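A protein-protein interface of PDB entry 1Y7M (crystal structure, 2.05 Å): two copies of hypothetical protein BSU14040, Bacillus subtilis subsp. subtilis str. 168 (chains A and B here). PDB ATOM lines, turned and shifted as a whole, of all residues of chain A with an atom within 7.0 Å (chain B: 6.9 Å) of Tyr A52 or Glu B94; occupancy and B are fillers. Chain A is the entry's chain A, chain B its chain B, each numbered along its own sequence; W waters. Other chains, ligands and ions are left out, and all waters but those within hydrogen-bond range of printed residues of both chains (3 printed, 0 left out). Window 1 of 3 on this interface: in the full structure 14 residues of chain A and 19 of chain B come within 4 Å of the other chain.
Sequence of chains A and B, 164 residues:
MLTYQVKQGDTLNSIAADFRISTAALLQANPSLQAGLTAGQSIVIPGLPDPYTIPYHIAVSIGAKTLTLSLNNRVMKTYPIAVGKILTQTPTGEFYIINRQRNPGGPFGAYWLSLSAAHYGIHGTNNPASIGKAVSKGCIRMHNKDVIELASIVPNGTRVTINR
The side-chain hydroxyl of Tyr A52 sits at hydrogen-bond distance from the side-chain hydroxyl of Thr B161, at 3.4 Å. The side-chain hydroxyl of Tyr A52 is in hydrogen-bond range of the side-chain carboxylate of Glu B94 (2.6 Å). The side-chain carboxylate of Asp A50 lies within hydrogen-bond range of the side-chain amide nitrogen of Asn B73, 3.3 Å away.
Water W2 lies within hydrogen-bond range of OD1 of Asn B73 (2.6 Å), ND1 of His B57 (2.7 Å) and OG1 of Thr A3 (3.4 Å). Water W3 lies within hydrogen-bond range of OE2 of Glu B94 (2.6 Å) and NH1 of Arg A159 (3.1 Å). Water W1 lies within hydrogen-bond range of the guanidinium group of Arg B159 (3.1 Å) and the backbone carbonyl oxygen of Tyr A52 (3.5 Å).
O of Asp A50 lies within hydrogen-bond range of OG1 of Thr A53. OH of Tyr B96 is in hydrogen-bond range of NH1 of Arg B159, at 3.3 Å. The backbone carbonyl oxygen of Arg B159 sits at hydrogen-bond distance from the backbone NH of Ile B58, at 2.9 Å. NE2 of His B57 is in hydrogen-bond range of OG1 of Thr B161, 2.8 Å away. The side-chain carboxylate (OE1) of Glu B94 sits at hydrogen-bond distance from the side-chain hydroxyl (OG1) of Thr B161 (2.6 Å). O of Ile B58 lies within hydrogen-bond range of N of Thr B161, 2.8 Å away.
Printed residues of chain B within 4 Å of Thr A3: Asn B73 (3.4 Å). Of chain B, only Glu B94, Arg B159 and Thr B161 come within 4 Å of Tyr A52. Printed residues of chain B within 4 Å of Thr A53: Tyr B52. Printed residues of chain A within 4 Å of Glu B94: Tyr A52. Of the printed residues of chain A, Arg B159 touches Tyr A52. Printed residues of chain A within 4 Å of Thr B161: Tyr A52 (3.4 Å). The nearest residue of chain A that does not touch Glu B94 is Arg A159 (4.2 Å). The nearest printed residue of chain B that does not touch Thr A3 is His B57 (4.7 Å).
Among the printed residues, pairs that only touch across the chains: Thr A53 with Tyr B52 (3.2 Å), Thr A3 with Asn B73 (3.4 Å) and Tyr A52 with Arg B159 (3.4 Å).
Of the 15 printed residues of chain B, 5 touch a printed residue of chain A. Printed residues of chain B that touch a printed residue of chain A: Tyr B52, Asn B73, Glu B94, Arg B159 and Thr B161. Hydrophobic or aromatic side chains of chain B that line the printed part of chain A: Tyr B52. Of the 13 printed residues of chain A, 4 touch a printed residue of chain B. Hydrophobic or aromatic side chains of chain A within 4 Å of the printed part of chain B: Tyr A52. Among the printed residues, 6 pairs touch across the chains. Among the printed residues, no Asp or Glu carboxylate lies within 4 Å of a Lys or Arg side-chain nitrogen of the other chain.
Tyr A52 touches Glu B94, but with the chains exchanged Glu A94 does not touch Tyr B52 (15.8 Å). Tyr A52 touches Arg B159, but with the chains exchanged Arg A159 does not touch Tyr B52 (9.2 Å). Positions printed for both chains: 52, 57, 94, 96 and 159. Of the 6 pairs that touch across the chains among the printed residues, none has its exchanged pair printed and touching as well.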
ATOM      1  N   THR A   3      10.228   6.494 -26.977  1.00  0.00           N
ATOM      2  CA  THR A   3       9.415   6.248 -28.153  1.00  0.00           C
ATOM      3  C   THR A   3      10.296   6.108 -29.368  1.00  0.00           C
ATOM      4  O   THR A   3      11.213   6.909 -29.605  1.00  0.00           O
ATOM      5  CB  THR A   3       8.375   7.378 -28.378  1.00  0.00           C
ATOM      6  OG1 THR A   3       8.987   8.508 -29.013  1.00  0.00           O
ATOM      7  CG2 THR A   3       7.876   7.931 -27.072  1.00  0.00           C
ATOM      8  N   PRO A  49      13.835   5.230 -19.949  1.00  0.00           N
ATOM      9  CA  PRO A  49      13.335   6.604 -19.805  1.00  0.00           C
ATOM     10  C   PRO A  49      13.314   7.327 -21.150  1.00  0.00           C
ATOM     11  O   PRO A  49      13.919   6.872 -22.117  1.00  0.00           O
ATOM     12  CB  PRO A  49      14.357   7.248 -18.863  1.00  0.00           C
ATOM     13  CG  PRO A  49      15.568   6.558 -19.164  1.00  0.00           C
ATOM     14  CD  PRO A  49      15.174   5.088 -19.346  1.00  0.00           C
ATOM     15  N   ASP A  50      12.602   8.438 -21.204  1.00  0.00           N
ATOM     16  CA  ASP A  50      12.593   9.290 -22.380  1.00  0.00           C
ATOM     17  C   ASP A  50      14.010   9.875 -22.516  1.00  0.00           C
ATOM     18  O   ASP A  50      14.492  10.534 -21.607  1.00  0.00           O
ATOM     19  CB  ASP A  50      11.546  10.397 -22.207  1.00  0.00           C
ATOM     20  CG  ASP A  50      11.488  11.363 -23.386  1.00  0.00           C
ATOM     21  OD1 ASP A  50      12.366  11.339 -24.250  1.00  0.00           O
ATOM     22  OD2 ASP A  50      10.568  12.185 -23.544  1.00  0.00           O
ATOM     23  N   PRO A  51      14.683   9.621 -23.630  1.00  0.00           N
ATOM     24  CA  PRO A  51      16.095   9.983 -23.753  1.00  0.00           C
ATOM     25  C   PRO A  51      16.308  11.503 -23.824  1.00  0.00           C
ATOM     26  O   PRO A  51      17.424  11.944 -23.597  1.00  0.00           O
ATOM     27  CB  PRO A  51      16.504   9.284 -25.053  1.00  0.00           C
ATOM     28  CG  PRO A  51      15.259   9.250 -25.846  1.00  0.00           C
ATOM     29  CD  PRO A  51      14.178   9.006 -24.870  1.00  0.00           C
ATOM     30  N   TYR A  52      15.254  12.273 -24.110  1.00  0.00           N
ATOM     31  CA  TYR A  52      15.334  13.738 -24.100  1.00  0.00           C
ATOM     32  C   TYR A  52      15.360  14.301 -22.672  1.00  0.00           C
ATOM     33  O   TYR A  52      15.699  15.450 -22.474  1.00  0.00           O
ATOM     34  CB  TYR A  52      14.206  14.367 -24.946  1.00  0.00           C
ATOM     35  CG  TYR A  52      14.278  13.926 -26.384  1.00  0.00           C
ATOM     36  CD1 TYR A  52      13.377  13.005 -26.899  1.00  0.00           C
ATOM     37  CD2 TYR A  52      15.286  14.388 -27.221  1.00  0.00           C
ATOM     38  CE1 TYR A  52      13.473  12.573 -28.220  1.00  0.00           C
ATOM     39  CE2 TYR A  52      15.387  13.971 -28.526  1.00  0.00           C
ATOM     40  CZ  TYR A  52      14.473  13.062 -29.025  1.00  0.00           C
ATOM     41  OH  TYR A  52      14.568  12.634 -30.325  1.00  0.00           O
ATOM     42  N   THR A  53      15.052  13.477 -21.682  1.00  0.00           N
ATOM     43  CA  THR A  53      15.198  13.852 -20.271  1.00  0.00           C
ATOM     44  C   THR A  53      16.591  13.554 -19.713  1.00  0.00           C
ATOM     45  O   THR A  53      16.908  13.959 -18.596  1.00  0.00           O
ATOM     46  CB  THR A  53      14.169  13.097 -19.398  1.00  0.00           C
ATOM     47  OG1 THR A  53      14.419  11.679 -19.451  1.00  0.00           O
ATOM     48  CG2 THR A  53      12.775  13.261 -19.943  1.00  0.00           C
ATOM     49  N   ILE A  54      17.402  12.821 -20.468  1.00  0.00           N
ATOM     50  CA  ILE A  54      18.773  12.528 -20.080  1.00  0.00           C
ATOM     51  C   ILE A  54      19.623  13.616 -20.724  1.00  0.00           C
ATOM     52  O   ILE A  54      19.682  13.680 -21.944  1.00  0.00           O
ATOM     53  CB  ILE A  54      19.175  11.131 -20.573  1.00  0.00           C
ATOM     54  CG1 ILE A  54      18.515  10.053 -19.714  1.00  0.00           C
ATOM     55  CG2 ILE A  54      20.696  10.899 -20.540  1.00  0.00           C
ATOM     56  CD1 ILE A  54      18.267   8.792 -20.466  1.00  0.00           C
ATOM     57  N   PRO A  55      20.266  14.461 -19.912  1.00  0.00           N
ATOM     58  CA  PRO A  55      21.053  15.598 -20.419  1.00  0.00           C
ATOM     59  C   PRO A  55      22.407  15.173 -21.021  1.00  0.00           C
ATOM     60  O   PRO A  55      23.137  16.024 -21.553  1.00  0.00           O
ATOM     61  CB  PRO A  55      21.252  16.463 -19.169  1.00  0.00           C
ATOM     62  CG  PRO A  55      21.231  15.453 -18.006  1.00  0.00           C
ATOM     63  CD  PRO A  55      20.322  14.370 -18.442  1.00  0.00           C
ATOM     64  N   HIS A  57      24.652  13.137 -23.852  1.00  0.00           N
ATOM     65  CA  HIS A  57      24.587  12.863 -25.267  1.00  0.00           C
ATOM     66  C   HIS A  57      25.986  12.406 -25.654  1.00  0.00           C
ATOM     67  O   HIS A  57      26.955  13.130 -25.443  1.00  0.00           O
ATOM     68  CB  HIS A  57      24.195  14.137 -26.050  1.00  0.00           C
ATOM     69  CG  HIS A  57      23.769  13.870 -27.458  1.00  0.00           C
ATOM     70  ND1 HIS A  57      22.562  14.286 -27.957  1.00  0.00           N
ATOM     71  CD2 HIS A  57      24.382  13.211 -28.469  1.00  0.00           C
ATOM     72  CE1 HIS A  57      22.439  13.881 -29.211  1.00  0.00           C
ATOM     73  NE2 HIS A  57      23.531  13.226 -29.547  1.00  0.00           N
ATOM     74  N   GLU A  94      21.463   7.222 -35.279  1.00  0.00           N
ATOM     75  CA  GLU A  94      21.040   7.502 -33.911  1.00  0.00           C
ATOM     76  C   GLU A  94      20.783   6.205 -33.180  1.00  0.00           C
ATOM     77  O   GLU A  94      19.990   5.384 -33.638  1.00  0.00           O
ATOM     78  CB  GLU A  94      19.754   8.307 -33.915  1.00  0.00           C
ATOM     79  CG  GLU A  94      19.893   9.683 -34.525  1.00  0.00           C
ATOM     80  CD  GLU A  94      20.831  10.615 -33.764  1.00  0.00           C
ATOM     81  OE1 GLU A  94      21.254  10.333 -32.620  1.00  0.00           O
ATOM     82  OE2 GLU A  94      21.131  11.657 -34.348  1.00  0.00           O
ATOM     83  N   TYR A  96      20.825   4.361 -28.850  1.00  0.00           N
ATOM     84  CA  TYR A  96      20.678   4.596 -27.424  1.00  0.00           C
ATOM     85  C   TYR A  96      21.501   3.571 -26.669  1.00  0.00           C
ATOM     86  O   TYR A  96      21.758   2.484 -27.184  1.00  0.00           O
ATOM     87  CB  TYR A  96      19.219   4.454 -27.033  1.00  0.00           C
ATOM     88  CG  TYR A  96      18.316   5.332 -27.845  1.00  0.00           C
ATOM     89  CD1 TYR A  96      17.588   4.812 -28.899  1.00  0.00           C
ATOM     90  CD2 TYR A  96      18.226   6.696 -27.583  1.00  0.00           C
ATOM     91  CE1 TYR A  96      16.777   5.602 -29.660  1.00  0.00           C
ATOM     92  CE2 TYR A  96      17.420   7.518 -28.359  1.00  0.00           C
ATOM     93  CZ  TYR A  96      16.691   6.960 -29.395  1.00  0.00           C
ATOM     94  OH  TYR A  96      15.883   7.737 -30.185  1.00  0.00           O
ATOM     95  N   GLY A 157      19.349   4.639 -21.819  1.00  0.00           N
ATOM     96  CA  GLY A 157      18.495   5.594 -22.509  1.00  0.00           C
ATOM     97  C   GLY A 157      19.274   6.731 -23.193  1.00  0.00           C
ATOM     98  O   GLY A 157      18.754   7.391 -24.102  1.00  0.00           O
ATOM     99  N   ARG A 159      21.396   9.028 -25.434  1.00  0.00           N
ATOM    100  CA  ARG A 159      21.546   9.087 -26.880  1.00  0.00           C
ATOM    101  C   ARG A 159      22.997   8.934 -27.294  1.00  0.00           C
ATOM    102  O   ARG A 159      23.889   9.539 -26.686  1.00  0.00           O
ATOM    103  CB  ARG A 159      21.012  10.403 -27.412  1.00  0.00           C
ATOM    104  CG  ARG A 159      19.503  10.526 -27.326  1.00  0.00           C
ATOM    105  CD  ARG A 159      19.009  11.772 -28.013  1.00  0.00           C
ATOM    106  NE  ARG A 159      19.175  12.946 -27.174  1.00  0.00           N
ATOM    107  CZ  ARG A 159      19.242  14.214 -27.613  1.00  0.00           C
ATOM    108  NH1 ARG A 159      19.186  14.516 -28.910  1.00  0.00           N
ATOM    109  NH2 ARG A 159      19.376  15.187 -26.729  1.00  0.00           N
ATOM    110  N   TYR B  52      12.147  20.774 -24.052  1.00  0.00           N
ATOM    111  CA  TYR B  52      11.588  19.840 -23.076  1.00  0.00           C
ATOM    112  C   TYR B  52      10.380  20.395 -22.322  1.00  0.00           C
ATOM    113  O   TYR B  52       9.600  19.617 -21.777  1.00  0.00           O
ATOM    114  CB  TYR B  52      12.624  19.304 -22.076  1.00  0.00           C
ATOM    115  CG  TYR B  52      12.031  18.156 -21.283  1.00  0.00           C
ATOM    116  CD1 TYR B  52      11.633  16.983 -21.927  1.00  0.00           C
ATOM    117  CD2 TYR B  52      11.773  18.273 -19.918  1.00  0.00           C
ATOM    118  CE1 TYR B  52      11.049  15.943 -21.232  1.00  0.00           C
ATOM    119  CE2 TYR B  52      11.188  17.232 -19.208  1.00  0.00           C
ATOM    120  CZ  TYR B  52      10.825  16.066 -19.871  1.00  0.00           C
ATOM    121  OH  TYR B  52      10.240  15.015 -19.183  1.00  0.00           O
ATOM    122  N   HIS B  57       5.828  16.584 -29.630  1.00  0.00           N
ATOM    123  CA  HIS B  57       6.986  16.077 -30.361  1.00  0.00           C
ATOM    124  C   HIS B  57       6.541  15.639 -31.754  1.00  0.00           C
ATOM    125  O   HIS B  57       5.605  14.860 -31.900  1.00  0.00           O
ATOM    126  CB  HIS B  57       7.605  14.899 -29.633  1.00  0.00           C
ATOM    127  CG  HIS B  57       8.833  14.349 -30.302  1.00  0.00           C
ATOM    128  ND1 HIS B  57       9.270  13.055 -30.102  1.00  0.00           N
ATOM    129  CD2 HIS B  57       9.710  14.912 -31.171  1.00  0.00           C
ATOM    130  CE1 HIS B  57      10.376  12.855 -30.799  1.00  0.00           C
ATOM    131  NE2 HIS B  57      10.663  13.965 -31.462  1.00  0.00           N
ATOM    132  N   ILE B  58       7.194  16.182 -32.779  1.00  0.00           N
ATOM    133  CA  ILE B  58       6.924  15.834 -34.155  1.00  0.00           C
ATOM    134  C   ILE B  58       8.013  14.860 -34.603  1.00  0.00           C
ATOM    135  O   ILE B  58       9.184  15.006 -34.254  1.00  0.00           O
ATOM    136  CB  ILE B  58       6.870  17.111 -35.021  1.00  0.00           C
ATOM    137  CG1 ILE B  58       5.673  17.956 -34.597  1.00  0.00           C
ATOM    138  CG2 ILE B  58       6.746  16.778 -36.481  1.00  0.00           C
ATOM    139  CD1 ILE B  58       5.669  19.338 -35.171  1.00  0.00           C
ATOM    140  N   ASN B  73       4.224  11.814 -25.547  1.00  0.00           N
ATOM    141  CA  ASN B  73       4.571  10.526 -26.160  1.00  0.00           C
ATOM    142  C   ASN B  73       3.389   9.573 -26.425  1.00  0.00           C
ATOM    143  O   ASN B  73       3.521   8.329 -26.351  1.00  0.00           O
ATOM    144  CB  ASN B  73       5.683   9.863 -25.335  1.00  0.00           C
ATOM    145  CG  ASN B  73       6.981  10.680 -25.353  1.00  0.00           C
ATOM    146  OD1 ASN B  73       7.346  11.286 -26.377  1.00  0.00           O
ATOM    147  ND2 ASN B  73       7.679  10.696 -24.226  1.00  0.00           N
ATOM    148  N   THR B  92      18.136  14.768 -42.271  1.00  0.00           N
ATOM    149  CA  THR B  92      17.746  14.054 -41.048  1.00  0.00           C
ATOM    150  C   THR B  92      18.405  14.622 -39.797  1.00  0.00           C
ATOM    151  O   THR B  92      19.432  15.272 -39.864  1.00  0.00           O
ATOM    152  CB  THR B  92      18.073  12.566 -41.160  1.00  0.00           C
ATOM    153  OG1 THR B  92      19.470  12.356 -41.400  1.00  0.00           O
ATOM    154  CG2 THR B  92      17.409  11.969 -42.380  1.00  0.00           C
ATOM    155  N   GLY B  93      17.792  14.345 -38.659  1.00  0.00           N
ATOM    156  CA  GLY B  93      18.332  14.706 -37.362  1.00  0.00           C
ATOM    157  C   GLY B  93      17.311  15.462 -36.545  1.00  0.00           C
ATOM    158  O   GLY B  93      16.100  15.371 -36.807  1.00  0.00           O
ATOM    159  N   GLU B  94      17.792  16.200 -35.552  1.00  0.00           N
ATOM    160  CA  GLU B  94      16.932  16.914 -34.626  1.00  0.00           C
ATOM    161  C   GLU B  94      16.860  18.368 -35.055  1.00  0.00           C
ATOM    162  O   GLU B  94      17.897  19.003 -35.206  1.00  0.00           O
ATOM    163  CB  GLU B  94      17.500  16.829 -33.213  1.00  0.00           C
ATOM    164  CG  GLU B  94      17.653  15.403 -32.678  1.00  0.00           C
ATOM    165  CD  GLU B  94      16.329  14.728 -32.369  1.00  0.00           C
ATOM    166  OE1 GLU B  94      15.271  15.386 -32.427  1.00  0.00           O
ATOM    167  OE2 GLU B  94      16.339  13.514 -32.053  1.00  0.00           O
ATOM    168  N   PHE B  95      15.637  18.861 -35.273  1.00  0.00           N
ATOM    169  CA  PHE B  95      15.367  20.271 -35.551  1.00  0.00           C
ATOM    170  C   PHE B  95      14.314  20.795 -34.571  1.00  0.00           C
ATOM    171  O   PHE B  95      13.805  20.060 -33.714  1.00  0.00           O
ATOM    172  CB  PHE B  95      14.907  20.429 -37.009  1.00  0.00           C
ATOM    173  CG  PHE B  95      15.877  19.834 -37.995  1.00  0.00           C
ATOM    174  CD1 PHE B  95      15.793  18.495 -38.349  1.00  0.00           C
ATOM    175  CD2 PHE B  95      16.931  20.600 -38.504  1.00  0.00           C
ATOM    176  CE1 PHE B  95      16.703  17.930 -39.233  1.00  0.00           C
ATOM    177  CE2 PHE B  95      17.849  20.045 -39.379  1.00  0.00           C
ATOM    178  CZ  PHE B  95      17.725  18.706 -39.758  1.00  0.00           C
ATOM    179  N   TYR B  96      14.008  22.074 -34.706  1.00  0.00           N
ATOM    180  CA  TYR B  96      12.994  22.745 -33.926  1.00  0.00           C
ATOM    181  C   TYR B  96      12.243  23.686 -34.842  1.00  0.00           C
ATOM    182  O   TYR B  96      12.803  24.222 -35.812  1.00  0.00           O
ATOM    183  CB  TYR B  96      13.624  23.527 -32.773  1.00  0.00           C
ATOM    184  CG  TYR B  96      14.584  22.713 -31.951  1.00  0.00           C
ATOM    185  CD1 TYR B  96      14.123  21.947 -30.895  1.00  0.00           C
ATOM    186  CD2 TYR B  96      15.950  22.674 -32.249  1.00  0.00           C
ATOM    187  CE1 TYR B  96      14.977  21.164 -30.157  1.00  0.00           C
ATOM    188  CE2 TYR B  96      16.828  21.886 -31.491  1.00  0.00           C
ATOM    189  CZ  TYR B  96      16.306  21.124 -30.451  1.00  0.00           C
ATOM    190  OH  TYR B  96      17.098  20.328 -29.644  1.00  0.00           O
ATOM    191  N   SER B 116      14.981  24.660 -37.895  1.00  0.00           N
ATOM    192  CA  SER B 116      16.304  25.135 -37.472  1.00  0.00           C
ATOM    193  C   SER B 116      17.482  24.717 -38.397  1.00  0.00           C
ATOM    194  O   SER B 116      18.570  24.421 -37.915  1.00  0.00           O
ATOM    195  CB  SER B 116      16.579  24.654 -36.050  1.00  0.00           C
ATOM    196  OG  SER B 116      16.484  23.244 -35.972  1.00  0.00           O
ATOM    197  N   ARG B 159      10.249  20.340 -30.807  1.00  0.00           N
ATOM    198  CA  ARG B 159      11.126  19.371 -31.451  1.00  0.00           C
ATOM    199  C   ARG B 159      10.493  18.670 -32.666  1.00  0.00           C
ATOM    200  O   ARG B 159       9.343  18.186 -32.632  1.00  0.00           O
ATOM    201  CB  ARG B 159      11.580  18.338 -30.421  1.00  0.00           C
ATOM    202  CG  ARG B 159      12.589  17.357 -30.923  1.00  0.00           C
ATOM    203  CD  ARG B 159      13.072  16.385 -29.871  1.00  0.00           C
ATOM    204  NE  ARG B 159      13.756  17.006 -28.740  1.00  0.00           N
ATOM    205  CZ  ARG B 159      15.014  17.429 -28.747  1.00  0.00           C
ATOM    206  NH1 ARG B 159      15.779  17.312 -29.833  1.00  0.00           N
ATOM    207  NH2 ARG B 159      15.518  17.969 -27.648  1.00  0.00           N
ATOM    208  N   VAL B 160      11.283  18.593 -33.729  1.00  0.00           N
ATOM    209  CA  VAL B 160      10.933  17.909 -34.962  1.00  0.00           C
ATOM    210  C   VAL B 160      12.073  16.932 -35.211  1.00  0.00           C
ATOM    211  O   VAL B 160      13.182  17.359 -35.480  1.00  0.00           O
ATOM    212  CB  VAL B 160      10.791  18.918 -36.110  1.00  0.00           C
ATOM    213  CG1 VAL B 160      10.516  18.206 -37.463  1.00  0.00           C
ATOM    214  CG2 VAL B 160       9.644  19.904 -35.813  1.00  0.00           C
ATOM    215  N   THR B 161      11.838  15.631 -35.026  1.00  0.00           N
ATOM    216  CA  THR B 161      12.859  14.636 -35.329  1.00  0.00           C
ATOM    217  C   THR B 161      12.578  14.057 -36.697  1.00  0.00           C
ATOM    218  O   THR B 161      11.463  13.609 -36.949  1.00  0.00           O
ATOM    219  CB  THR B 161      12.865  13.517 -34.285  1.00  0.00           C
ATOM    220  OG1 THR B 161      13.045  14.078 -32.984  1.00  0.00           O
ATOM    221  CG2 THR B 161      14.078  12.581 -34.464  1.00  0.00           C
ATOM    222  N   ILE B 162      13.574  14.110 -37.583  1.00  0.00           N
ATOM    223  CA  ILE B 162      13.466  13.568 -38.937  1.00  0.00           C
ATOM    224  C   ILE B 162      14.371  12.333 -39.098  1.00  0.00           C
ATOM    225  O   ILE B 162      15.578  12.395 -38.872  1.00  0.00           O
ATOM    226  CB  ILE B 162      13.810  14.662 -40.005  1.00  0.00           C
ATOM    227  CG1 ILE B 162      12.903  15.892 -39.827  1.00  0.00           C
ATOM    228  CG2 ILE B 162      13.641  14.085 -41.401  1.00  0.00           C
ATOM    229  CD1 ILE B 162      13.189  17.037 -40.779  1.00  0.00           C
ATOM    230  N   ASN B 163      13.751  11.220 -39.488  1.00  0.00           N
ATOM    231  CA  ASN B 163      14.402   9.927 -39.720  1.00  0.00           C
ATOM    232  C   ASN B 163      14.236   9.564 -41.192  1.00  0.00           C
ATOM    233  O   ASN B 163      13.333  10.053 -41.837  1.00  0.00           O
ATOM    234  CB  ASN B 163      13.683   8.855 -38.879  1.00  0.00           C
ATOM    235  CG  ASN B 163      13.652   9.191 -37.381  1.00  0.00           C
ATOM    236  OD1 ASN B 163      14.689   9.147 -36.717  1.00  0.00           O
ATOM    237  ND2 ASN B 163      12.468   9.539 -36.851  1.00  0.00           N
HETATM  238  O   HOH W   1      14.887  18.098 -24.579  1.00  0.00           O
HETATM  239  O   HOH W   2       7.400  11.470 -28.971  1.00  0.00           O
HETATM  240  O   HOH W   3      18.467  12.341 -31.018  1.00  0.00           O
